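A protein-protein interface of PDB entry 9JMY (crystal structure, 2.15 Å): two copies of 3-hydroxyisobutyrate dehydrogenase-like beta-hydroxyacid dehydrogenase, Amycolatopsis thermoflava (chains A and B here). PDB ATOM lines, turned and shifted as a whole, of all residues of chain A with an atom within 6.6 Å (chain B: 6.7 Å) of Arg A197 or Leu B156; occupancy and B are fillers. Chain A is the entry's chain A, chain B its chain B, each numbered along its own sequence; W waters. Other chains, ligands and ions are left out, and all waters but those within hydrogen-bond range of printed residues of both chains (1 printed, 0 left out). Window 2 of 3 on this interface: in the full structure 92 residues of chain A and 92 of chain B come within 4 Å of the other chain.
The side-chain carboxylate of Asp A194 lies within salt-bridge range of the guanidinium group of Arg B221, at 2.4 Å.
The backbone NH of Ala A193 is in hydrogen-bond range of the backbone carbonyl oxygen of Leu A188, at 3.0 Å.
N of Ala A196 lies within hydrogen-bond range of OD1 of Asp A194 (2.9 Å).
The backbone carbonyl oxygen (O) of Glu B154 sits at hydrogen-bond distance from the backbone NH (N) of Tyr B133.
The backbone carbonyl oxygen (O) of Tyr B133 sits at hydrogen-bond distance from the backbone NH (N) of Leu B156 (2.7 Å).
Val B217 touches Phe A185.
Leu B165 touches Leu A188 (CG to CD2, 3.7 Å).
CD1 of Leu A188 touches CZ of Phe B166 (3.6 Å).
CG2 of Val B217 touches CA of Ala A196, at 3.8 Å.
CB of Ala A196 touches NH1 of Arg B221, at 3.96 Å.
Arg A197 touches Leu B156.
CZ of Phe B166 touches CB of Arg A197, at 3.8 Å.
CG2 of Val B217 touches CG2 of Val A199, at 3.2 Å.
CD1 of Phe A201 touches CZ of Phe B132, at 3.8 Å.
Phe A201 touches Glu B154.
Of the printed residues of chain B, Phe A185 touches Val B217 (3.9 Å).
Ala A193 touches none of the printed residues of chain B.
Of chain B, only Leu B156 (3.8 Å) and Phe B166 (3.8 Å) come within 4 Å of Arg A197.
Printed residues of chain B within 4 Å of Val A199: Val B217.
Of the printed residues of chain A, Phe B132 touches Phe A201.
Leu B156 touches just one residue of chain A: Arg A197.
Leu B162 touches none of the printed residues of chain A.
Printed residues of chain A within 4 Å of Leu B165: Leu A188 (3.7 Å).
Of the printed residues of chain A, Val B217 touches Phe A185, Ala A196 and Val A199.
The nearest printed residue of chain B that does not touch Phe A201 is Phe B166 (5.1 Å).
Of the 11 printed residues of chain A, 7 touch a printed residue of chain B.
Printed residues of chain A that touch a printed residue of chain B: Phe A185, Leu A188, Asp A194, Ala A196, Arg A197, Val A199 and Phe A201.
Hydrophobic or aromatic side chains of chain A within 4 Å of the printed part of chain B: Phe A185, Leu A188, Ala A196, Val A199 and Phe A201.
Along chain A the printed residues that touch a printed residue of chain B span positions 185 to 201.
Of the 19 printed residues of chain B, 7 touch a printed residue of chain A.
Hydrophobic or aromatic side chains of chain B that line the printed part of chain A: Phe B132, Leu B156, Leu B165, Phe B166 and Val B217.
Among the printed residues, 11 pairs touch across the chains.
No position is printed for both chains.
Water W1 lies within hydrogen-bond range of NH2 of Arg A197 (2.9 Å) and OE2 of Glu B154 (3.2 Å).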
ATOM      1  N   PHE A 185     -25.643  21.237  -7.850  1.00  0.00           N
ATOM      2  CA  PHE A 185     -24.219  21.476  -8.163  1.00  0.00           C
ATOM      3  C   PHE A 185     -24.064  22.903  -8.695  1.00  0.00           C
ATOM      4  O   PHE A 185     -23.083  23.554  -8.343  1.00  0.00           O
ATOM      5  CB  PHE A 185     -23.679  20.408  -9.120  1.00  0.00           C
ATOM      6  CG  PHE A 185     -23.495  19.034  -8.531  1.00  0.00           C
ATOM      7  CD1 PHE A 185     -23.381  18.832  -7.164  1.00  0.00           C
ATOM      8  CD2 PHE A 185     -23.431  17.927  -9.362  1.00  0.00           C
ATOM      9  CE1 PHE A 185     -23.220  17.558  -6.644  1.00  0.00           C
ATOM     10  CE2 PHE A 185     -23.250  16.653  -8.837  1.00  0.00           C
ATOM     11  CZ  PHE A 185     -23.149  16.468  -7.479  1.00  0.00           C
ATOM     12  N   LEU A 188     -24.074  25.551  -5.835  1.00  0.00           N
ATOM     13  CA  LEU A 188     -22.766  25.515  -5.124  1.00  0.00           C
ATOM     14  C   LEU A 188     -21.721  26.237  -5.985  1.00  0.00           C
ATOM     15  O   LEU A 188     -21.111  27.217  -5.503  1.00  0.00           O
ATOM     16  CB  LEU A 188     -22.330  24.067  -4.894  1.00  0.00           C
ATOM     17  CG  LEU A 188     -22.975  23.269  -3.758  1.00  0.00           C
ATOM     18  CD1 LEU A 188     -21.922  22.727  -2.809  1.00  0.00           C
ATOM     19  CD2 LEU A 188     -24.037  24.046  -3.015  1.00  0.00           C
ATOM     20  N   ALA A 193     -18.372  27.471  -4.209  1.00  0.00           N
ATOM     21  CA  ALA A 193     -18.101  26.211  -3.471  1.00  0.00           C
ATOM     22  C   ALA A 193     -17.937  25.074  -4.485  1.00  0.00           C
ATOM     23  O   ALA A 193     -18.501  25.174  -5.587  1.00  0.00           O
ATOM     24  CB  ALA A 193     -19.187  25.911  -2.464  1.00  0.00           C
ATOM     25  N   ASP A 194     -17.160  24.062  -4.114  1.00  0.00           N
ATOM     26  CA  ASP A 194     -16.878  22.871  -4.950  1.00  0.00           C
ATOM     27  C   ASP A 194     -18.071  21.918  -4.908  1.00  0.00           C
ATOM     28  O   ASP A 194     -18.345  21.337  -3.863  1.00  0.00           O
ATOM     29  CB  ASP A 194     -15.617  22.135  -4.492  1.00  0.00           C
ATOM     30  CG  ASP A 194     -15.174  21.089  -5.506  1.00  0.00           C
ATOM     31  OD1 ASP A 194     -16.028  20.595  -6.303  1.00  0.00           O
ATOM     32  OD2 ASP A 194     -13.968  20.805  -5.537  1.00  0.00           O
ATOM     33  N   PRO A 195     -18.768  21.686  -6.047  1.00  0.00           N
ATOM     34  CA  PRO A 195     -19.927  20.797  -6.075  1.00  0.00           C
ATOM     35  C   PRO A 195     -19.620  19.397  -5.532  1.00  0.00           C
ATOM     36  O   PRO A 195     -20.560  18.745  -5.057  1.00  0.00           O
ATOM     37  CB  PRO A 195     -20.348  20.700  -7.561  1.00  0.00           C
ATOM     38  CG  PRO A 195     -19.632  21.846  -8.263  1.00  0.00           C
ATOM     39  CD  PRO A 195     -18.509  22.309  -7.355  1.00  0.00           C
ATOM     40  N   ALA A 196     -18.355  18.963  -5.647  1.00  0.00           N
ATOM     41  CA  ALA A 196     -17.864  17.645  -5.194  1.00  0.00           C
ATOM     42  C   ALA A 196     -18.053  17.516  -3.680  1.00  0.00           C
ATOM     43  O   ALA A 196     -18.202  16.388  -3.223  1.00  0.00           O
ATOM     44  CB  ALA A 196     -16.417  17.432  -5.560  1.00  0.00           C
ATOM     45  N   ARG A 197     -18.048  18.627  -2.943  1.00  0.00           N
ATOM     46  CA  ARG A 197     -18.282  18.642  -1.473  1.00  0.00           C
ATOM     47  C   ARG A 197     -19.692  18.111  -1.141  1.00  0.00           C
ATOM     48  O   ARG A 197     -19.856  17.531  -0.050  1.00  0.00           O
ATOM     49  CB  ARG A 197     -18.111  20.066  -0.943  1.00  0.00           C
ATOM     50  CG  ARG A 197     -16.703  20.620  -1.111  1.00  0.00           C
ATOM     51  CD  ARG A 197     -16.400  21.732  -0.121  1.00  0.00           C
ATOM     52  NE  ARG A 197     -16.497  21.241   1.251  1.00  0.00           N
ATOM     53  CZ  ARG A 197     -16.555  22.006   2.337  1.00  0.00           C
ATOM     54  NH1 ARG A 197     -16.522  23.325   2.237  1.00  0.00           N
ATOM     55  NH2 ARG A 197     -16.641  21.440   3.527  1.00  0.00           N
ATOM     56  N   LEU A 198     -20.674  18.304  -2.032  1.00  0.00           N
ATOM     57  CA  LEU A 198     -22.087  17.910  -1.783  1.00  0.00           C
ATOM     58  C   LEU A 198     -22.257  16.393  -1.919  1.00  0.00           C
ATOM     59  O   LEU A 198     -23.175  15.871  -1.267  1.00  0.00           O
ATOM     60  CB  LEU A 198     -23.031  18.655  -2.735  1.00  0.00           C
ATOM     61  CG  LEU A 198     -24.515  18.587  -2.351  1.00  0.00           C
ATOM     62  CD1 LEU A 198     -24.744  19.105  -0.939  1.00  0.00           C
ATOM     63  CD2 LEU A 198     -25.394  19.336  -3.347  1.00  0.00           C
ATOM     64  N   VAL A 199     -21.366  15.705  -2.643  1.00  0.00           N
ATOM     65  CA  VAL A 199     -21.651  14.355  -3.218  1.00  0.00           C
ATOM     66  C   VAL A 199     -22.193  13.419  -2.144  1.00  0.00           C
ATOM     67  O   VAL A 199     -23.260  12.866  -2.331  1.00  0.00           O
ATOM     68  CB  VAL A 199     -20.459  13.753  -3.992  1.00  0.00           C
ATOM     69  CG1 VAL A 199     -20.509  12.236  -4.096  1.00  0.00           C
ATOM     70  CG2 VAL A 199     -20.392  14.343  -5.389  1.00  0.00           C
ATOM     71  N   PRO A 200     -21.493  13.146  -1.027  1.00  0.00           N
ATOM     72  CA  PRO A 200     -21.992  12.163  -0.065  1.00  0.00           C
ATOM     73  C   PRO A 200     -23.313  12.598   0.586  1.00  0.00           C
ATOM     74  O   PRO A 200     -24.125  11.745   0.890  1.00  0.00           O
ATOM     75  CB  PRO A 200     -20.845  11.996   0.939  1.00  0.00           C
ATOM     76  CG  PRO A 200     -19.971  13.221   0.762  1.00  0.00           C
ATOM     77  CD  PRO A 200     -20.193  13.705  -0.653  1.00  0.00           C
ATOM     78  N   PHE A 201     -23.540  13.902   0.751  1.00  0.00           N
ATOM     79  CA  PHE A 201     -24.780  14.422   1.379  1.00  0.00           C
ATOM     80  C   PHE A 201     -25.941  14.292   0.393  1.00  0.00           C
ATOM     81  O   PHE A 201     -27.074  14.135   0.849  1.00  0.00           O
ATOM     82  CB  PHE A 201     -24.601  15.863   1.843  1.00  0.00           C
ATOM     83  CG  PHE A 201     -23.366  16.056   2.672  1.00  0.00           C
ATOM     84  CD1 PHE A 201     -23.362  15.716   4.007  1.00  0.00           C
ATOM     85  CD2 PHE A 201     -22.195  16.527   2.097  1.00  0.00           C
ATOM     86  CE1 PHE A 201     -22.215  15.868   4.773  1.00  0.00           C
ATOM     87  CE2 PHE A 201     -21.055  16.686   2.864  1.00  0.00           C
ATOM     88  CZ  PHE A 201     -21.065  16.348   4.200  1.00  0.00           C
ATOM     89  N   PHE B 132     -25.374  21.222   8.996  1.00  0.00           N
ATOM     90  CA  PHE B 132     -24.424  22.193   8.422  1.00  0.00           C
ATOM     91  C   PHE B 132     -24.383  23.393   9.357  1.00  0.00           C
ATOM     92  O   PHE B 132     -25.459  23.770   9.868  1.00  0.00           O
ATOM     93  CB  PHE B 132     -24.829  22.588   7.006  1.00  0.00           C
ATOM     94  CG  PHE B 132     -24.799  21.432   6.049  1.00  0.00           C
ATOM     95  CD1 PHE B 132     -23.611  20.748   5.824  1.00  0.00           C
ATOM     96  CD2 PHE B 132     -25.940  21.036   5.368  1.00  0.00           C
ATOM     97  CE1 PHE B 132     -23.562  19.703   4.914  1.00  0.00           C
ATOM     98  CE2 PHE B 132     -25.883  19.993   4.455  1.00  0.00           C
ATOM     99  CZ  PHE B 132     -24.697  19.318   4.244  1.00  0.00           C
ATOM    100  N   TYR B 133     -23.181  23.924   9.569  1.00  0.00           N
ATOM    101  CA  TYR B 133     -22.899  25.153  10.346  1.00  0.00           C
ATOM    102  C   TYR B 133     -21.889  25.998   9.563  1.00  0.00           C
ATOM    103  O   TYR B 133     -20.972  25.444   8.900  1.00  0.00           O
ATOM    104  CB  TYR B 133     -22.388  24.818  11.747  1.00  0.00           C
ATOM    105  CG  TYR B 133     -23.402  24.188  12.666  1.00  0.00           C
ATOM    106  CD1 TYR B 133     -24.408  24.942  13.264  1.00  0.00           C
ATOM    107  CD2 TYR B 133     -23.342  22.837  12.950  1.00  0.00           C
ATOM    108  CE1 TYR B 133     -25.341  24.361  14.103  1.00  0.00           C
ATOM    109  CE2 TYR B 133     -24.253  22.243  13.800  1.00  0.00           C
ATOM    110  CZ  TYR B 133     -25.250  23.009  14.381  1.00  0.00           C
ATOM    111  OH  TYR B 133     -26.141  22.398  15.207  1.00  0.00           O
ATOM    112  N   SER B 134     -22.060  27.313   9.648  1.00  0.00           N
ATOM    113  CA  SER B 134     -21.092  28.310   9.131  1.00  0.00           C
ATOM    114  C   SER B 134     -21.277  29.626   9.880  1.00  0.00           C
ATOM    115  O   SER B 134     -22.368  29.853  10.444  1.00  0.00           O
ATOM    116  CB  SER B 134     -21.223  28.472   7.647  1.00  0.00           C
ATOM    117  OG  SER B 134     -22.497  28.963   7.289  1.00  0.00           O
ATOM    118  N   GLY B 135     -20.226  30.446   9.897  1.00  0.00           N
ATOM    119  CA  GLY B 135     -20.064  31.576  10.831  1.00  0.00           C
ATOM    120  C   GLY B 135     -18.768  31.442  11.623  1.00  0.00           C
ATOM    121  O   GLY B 135     -17.952  30.571  11.322  1.00  0.00           O
ATOM    122  N   ARG B 137     -15.794  30.367  13.620  1.00  0.00           N
ATOM    123  CA  ARG B 137     -15.282  29.045  14.082  1.00  0.00           C
ATOM    124  C   ARG B 137     -15.177  29.028  15.613  1.00  0.00           C
ATOM    125  O   ARG B 137     -15.633  28.039  16.233  1.00  0.00           O
ATOM    126  CB  ARG B 137     -13.919  28.783  13.438  1.00  0.00           C
ATOM    127  CG  ARG B 137     -13.329  27.407  13.708  1.00  0.00           C
ATOM    128  CD  ARG B 137     -12.196  27.102  12.734  1.00  0.00           C
ATOM    129  NE  ARG B 137     -12.408  25.852  12.005  1.00  0.00           N
ATOM    130  CZ  ARG B 137     -12.093  25.639  10.727  1.00  0.00           C
ATOM    131  NH1 ARG B 137     -11.540  26.594   9.999  1.00  0.00           N
ATOM    132  NH2 ARG B 137     -12.347  24.467  10.168  1.00  0.00           N
ATOM    133  N   GLU B 154     -21.371  19.658  10.983  1.00  0.00           N
ATOM    134  CA  GLU B 154     -20.649  19.737   9.709  1.00  0.00           C
ATOM    135  C   GLU B 154     -20.344  21.214   9.482  1.00  0.00           C
ATOM    136  O   GLU B 154     -21.094  21.836   8.741  1.00  0.00           O
ATOM    137  CB  GLU B 154     -21.555  19.104   8.654  1.00  0.00           C
ATOM    138  CG  GLU B 154     -20.809  18.538   7.483  1.00  0.00           C
ATOM    139  CD  GLU B 154     -19.890  17.408   7.890  1.00  0.00           C
ATOM    140  OE1 GLU B 154     -20.376  16.418   8.501  1.00  0.00           O
ATOM    141  OE2 GLU B 154     -18.697  17.557   7.642  1.00  0.00           O
ATOM    142  N   TYR B 155     -19.316  21.737  10.155  1.00  0.00           N
ATOM    143  CA  TYR B 155     -18.862  23.147  10.093  1.00  0.00           C
ATOM    144  C   TYR B 155     -18.218  23.385   8.721  1.00  0.00           C
ATOM    145  O   TYR B 155     -17.250  22.712   8.412  1.00  0.00           O
ATOM    146  CB  TYR B 155     -17.888  23.475  11.236  1.00  0.00           C
ATOM    147  CG  TYR B 155     -17.370  24.888  11.162  1.00  0.00           C
ATOM    148  CD1 TYR B 155     -18.156  25.948  11.578  1.00  0.00           C
ATOM    149  CD2 TYR B 155     -16.147  25.180  10.573  1.00  0.00           C
ATOM    150  CE1 TYR B 155     -17.719  27.261  11.468  1.00  0.00           C
ATOM    151  CE2 TYR B 155     -15.700  26.487  10.452  1.00  0.00           C
ATOM    152  CZ  TYR B 155     -16.490  27.534  10.900  1.00  0.00           C
ATOM    153  OH  TYR B 155     -16.086  28.834  10.758  1.00  0.00           O
ATOM    154  N   LEU B 156     -18.728  24.320   7.918  1.00  0.00           N
ATOM    155  CA  LEU B 156     -18.320  24.432   6.491  1.00  0.00           C
ATOM    156  C   LEU B 156     -17.303  25.562   6.322  1.00  0.00           C
ATOM    157  O   LEU B 156     -16.573  25.552   5.323  1.00  0.00           O
ATOM    158  CB  LEU B 156     -19.550  24.687   5.627  1.00  0.00           C
ATOM    159  CG  LEU B 156     -20.615  23.594   5.649  1.00  0.00           C
ATOM    160  CD1 LEU B 156     -21.833  24.031   4.840  1.00  0.00           C
ATOM    161  CD2 LEU B 156     -20.053  22.274   5.119  1.00  0.00           C
ATOM    162  N   GLY B 157     -17.287  26.519   7.245  1.00  0.00           N
ATOM    163  CA  GLY B 157     -16.392  27.679   7.181  1.00  0.00           C
ATOM    164  C   GLY B 157     -17.062  28.913   7.734  1.00  0.00           C
ATOM    165  O   GLY B 157     -18.143  28.784   8.362  1.00  0.00           O
ATOM    166  N   GLU B 158     -16.462  30.067   7.450  1.00  0.00           N
ATOM    167  CA  GLU B 158     -16.705  31.370   8.124  1.00  0.00           C
ATOM    168  C   GLU B 158     -17.858  32.105   7.449  1.00  0.00           C
ATOM    169  O   GLU B 158     -18.606  32.808   8.161  1.00  0.00           O
ATOM    170  CB  GLU B 158     -15.431  32.214   8.061  1.00  0.00           C
ATOM    171  CG  GLU B 158     -14.401  31.817   9.098  1.00  0.00           C
ATOM    172  CD  GLU B 158     -14.657  32.387  10.483  1.00  0.00           C
ATOM    173  OE1 GLU B 158     -14.191  31.796  11.461  1.00  0.00           O
ATOM    174  OE2 GLU B 158     -15.315  33.413  10.577  1.00  0.00           O
ATOM    175  N   ASP B 159     -17.977  31.992   6.123  1.00  0.00           N
ATOM    176  CA  ASP B 159     -19.066  32.667   5.364  1.00  0.00           C
ATOM    177  C   ASP B 159     -20.384  32.118   5.904  1.00  0.00           C
ATOM    178  O   ASP B 159     -20.614  30.907   5.728  1.00  0.00           O
ATOM    179  CB  ASP B 159     -18.945  32.465   3.854  1.00  0.00           C
ATOM    180  CG  ASP B 159     -20.221  32.739   3.073  1.00  0.00           C
ATOM    181  OD1 ASP B 159     -21.072  33.521   3.544  1.00  0.00           O
ATOM    182  OD2 ASP B 159     -20.370  32.153   1.998  1.00  0.00           O
ATOM    183  N   LEU B 162     -22.800  29.799   3.831  1.00  0.00           N
ATOM    184  CA  LEU B 162     -22.381  28.432   3.407  1.00  0.00           C
ATOM    185  C   LEU B 162     -23.371  27.354   3.856  1.00  0.00           C
ATOM    186  O   LEU B 162     -23.721  26.509   3.011  1.00  0.00           O
ATOM    187  CB  LEU B 162     -20.993  28.110   3.957  1.00  0.00           C
ATOM    188  CG  LEU B 162     -19.826  28.613   3.115  1.00  0.00           C
ATOM    189  CD1 LEU B 162     -18.524  28.419   3.881  1.00  0.00           C
ATOM    190  CD2 LEU B 162     -19.788  27.897   1.772  1.00  0.00           C
ATOM    191  N   ALA B 163     -23.743  27.320   5.141  1.00  0.00           N
ATOM    192  CA  ALA B 163     -24.618  26.265   5.709  1.00  0.00           C
ATOM    193  C   ALA B 163     -25.953  26.271   4.960  1.00  0.00           C
ATOM    194  O   ALA B 163     -26.518  25.187   4.655  1.00  0.00           O
ATOM    195  CB  ALA B 163     -24.820  26.476   7.185  1.00  0.00           C
ATOM    196  N   GLN B 164     -26.441  27.467   4.696  1.00  0.00           N
ATOM    197  CA  GLN B 164     -27.719  27.725   3.996  1.00  0.00           C
ATOM    198  C   GLN B 164     -27.570  27.295   2.535  1.00  0.00           C
ATOM    199  O   GLN B 164     -28.484  26.625   2.024  1.00  0.00           O
ATOM    200  CB  GLN B 164     -28.052  29.210   4.127  1.00  0.00           C
ATOM    201  CG  GLN B 164     -29.467  29.561   3.729  1.00  0.00           C
ATOM    202  CD  GLN B 164     -30.463  29.053   4.741  1.00  0.00           C
ATOM    203  OE1 GLN B 164     -30.957  27.925   4.618  1.00  0.00           O
ATOM    204  NE2 GLN B 164     -30.807  29.905   5.696  1.00  0.00           N
ATOM    205  N   LEU B 165     -26.464  27.680   1.885  1.00  0.00           N
ATOM    206  CA  LEU B 165     -26.123  27.216   0.513  1.00  0.00           C
ATOM    207  C   LEU B 165     -26.235  25.689   0.468  1.00  0.00           C
ATOM    208  O   LEU B 165     -26.898  25.174  -0.413  1.00  0.00           O
ATOM    209  CB  LEU B 165     -24.707  27.666   0.150  1.00  0.00           C
ATOM    210  CG  LEU B 165     -24.246  27.276  -1.258  1.00  0.00           C
ATOM    211  CD1 LEU B 165     -25.067  28.005  -2.320  1.00  0.00           C
ATOM    212  CD2 LEU B 165     -22.758  27.566  -1.446  1.00  0.00           C
ATOM    213  N   PHE B 166     -25.593  24.991   1.404  1.00  0.00           N
ATOM    214  CA  PHE B 166     -25.551  23.504   1.404  1.00  0.00           C
ATOM    215  C   PHE B 166     -26.955  22.958   1.682  1.00  0.00           C
ATOM    216  O   PHE B 166     -27.332  21.945   1.063  1.00  0.00           O
ATOM    217  CB  PHE B 166     -24.487  23.002   2.375  1.00  0.00           C
ATOM    218  CG  PHE B 166     -23.138  22.850   1.734  1.00  0.00           C
ATOM    219  CD1 PHE B 166     -22.438  23.960   1.303  1.00  0.00           C
ATOM    220  CD2 PHE B 166     -22.566  21.593   1.589  1.00  0.00           C
ATOM    221  CE1 PHE B 166     -21.201  23.809   0.696  1.00  0.00           C
ATOM    222  CE2 PHE B 166     -21.327  21.444   0.990  1.00  0.00           C
ATOM    223  CZ  PHE B 166     -20.645  22.551   0.545  1.00  0.00           C
ATOM    224  N   TYR B 167     -27.721  23.646   2.540  1.00  0.00           N
ATOM    225  CA  TYR B 167     -29.106  23.254   2.902  1.00  0.00           C
ATOM    226  C   TYR B 167     -29.984  23.320   1.651  1.00  0.00           C
ATOM    227  O   TYR B 167     -30.711  22.352   1.375  1.00  0.00           O
ATOM    228  CB  TYR B 167     -29.694  24.129   4.009  1.00  0.00           C
ATOM    229  CG  TYR B 167     -31.028  23.601   4.470  1.00  0.00           C
ATOM    230  CD1 TYR B 167     -31.110  22.565   5.394  1.00  0.00           C
ATOM    231  CD2 TYR B 167     -32.198  24.073   3.910  1.00  0.00           C
ATOM    232  CE1 TYR B 167     -32.341  22.050   5.785  1.00  0.00           C
ATOM    233  CE2 TYR B 167     -33.433  23.594   4.305  1.00  0.00           C
ATOM    234  CZ  TYR B 167     -33.504  22.569   5.234  1.00  0.00           C
ATOM    235  OH  TYR B 167     -34.718  22.063   5.555  1.00  0.00           O
ATOM    236  N   VAL B 217     -20.248  15.057 -11.149  1.00  0.00           N
ATOM    237  CA  VAL B 217     -19.129  15.876 -10.603  1.00  0.00           C
ATOM    238  C   VAL B 217     -18.045  16.031 -11.670  1.00  0.00           C
ATOM    239  O   VAL B 217     -17.728  17.172 -12.037  1.00  0.00           O
ATOM    240  CB  VAL B 217     -18.545  15.230  -9.334  1.00  0.00           C
ATOM    241  CG1 VAL B 217     -17.070  15.550  -9.142  1.00  0.00           C
ATOM    242  CG2 VAL B 217     -19.345  15.623  -8.113  1.00  0.00           C
ATOM    243  N   ARG B 221     -17.371  19.436 -13.873  1.00  0.00           N
ATOM    244  CA  ARG B 221     -16.037  19.916 -13.444  1.00  0.00           C
ATOM    245  C   ARG B 221     -15.097  20.006 -14.657  1.00  0.00           C
ATOM    246  O   ARG B 221     -14.471  21.065 -14.820  1.00  0.00           O
ATOM    247  CB  ARG B 221     -15.606  18.926 -12.370  1.00  0.00           C
ATOM    248  CG  ARG B 221     -14.323  19.228 -11.630  1.00  0.00           C
ATOM    249  CD  ARG B 221     -14.107  18.053 -10.694  1.00  0.00           C
ATOM    250  NE  ARG B 221     -13.410  18.481  -9.503  1.00  0.00           N
ATOM    251  CZ  ARG B 221     -13.946  19.216  -8.540  1.00  0.00           C
ATOM    252  NH1 ARG B 221     -15.201  19.631  -8.622  1.00  0.00           N
ATOM    253  NH2 ARG B 221     -13.216  19.537  -7.491  1.00  0.00           N
HETATM  254  O   HOH W   1     -17.397  19.905   5.913  1.00  0.00           O
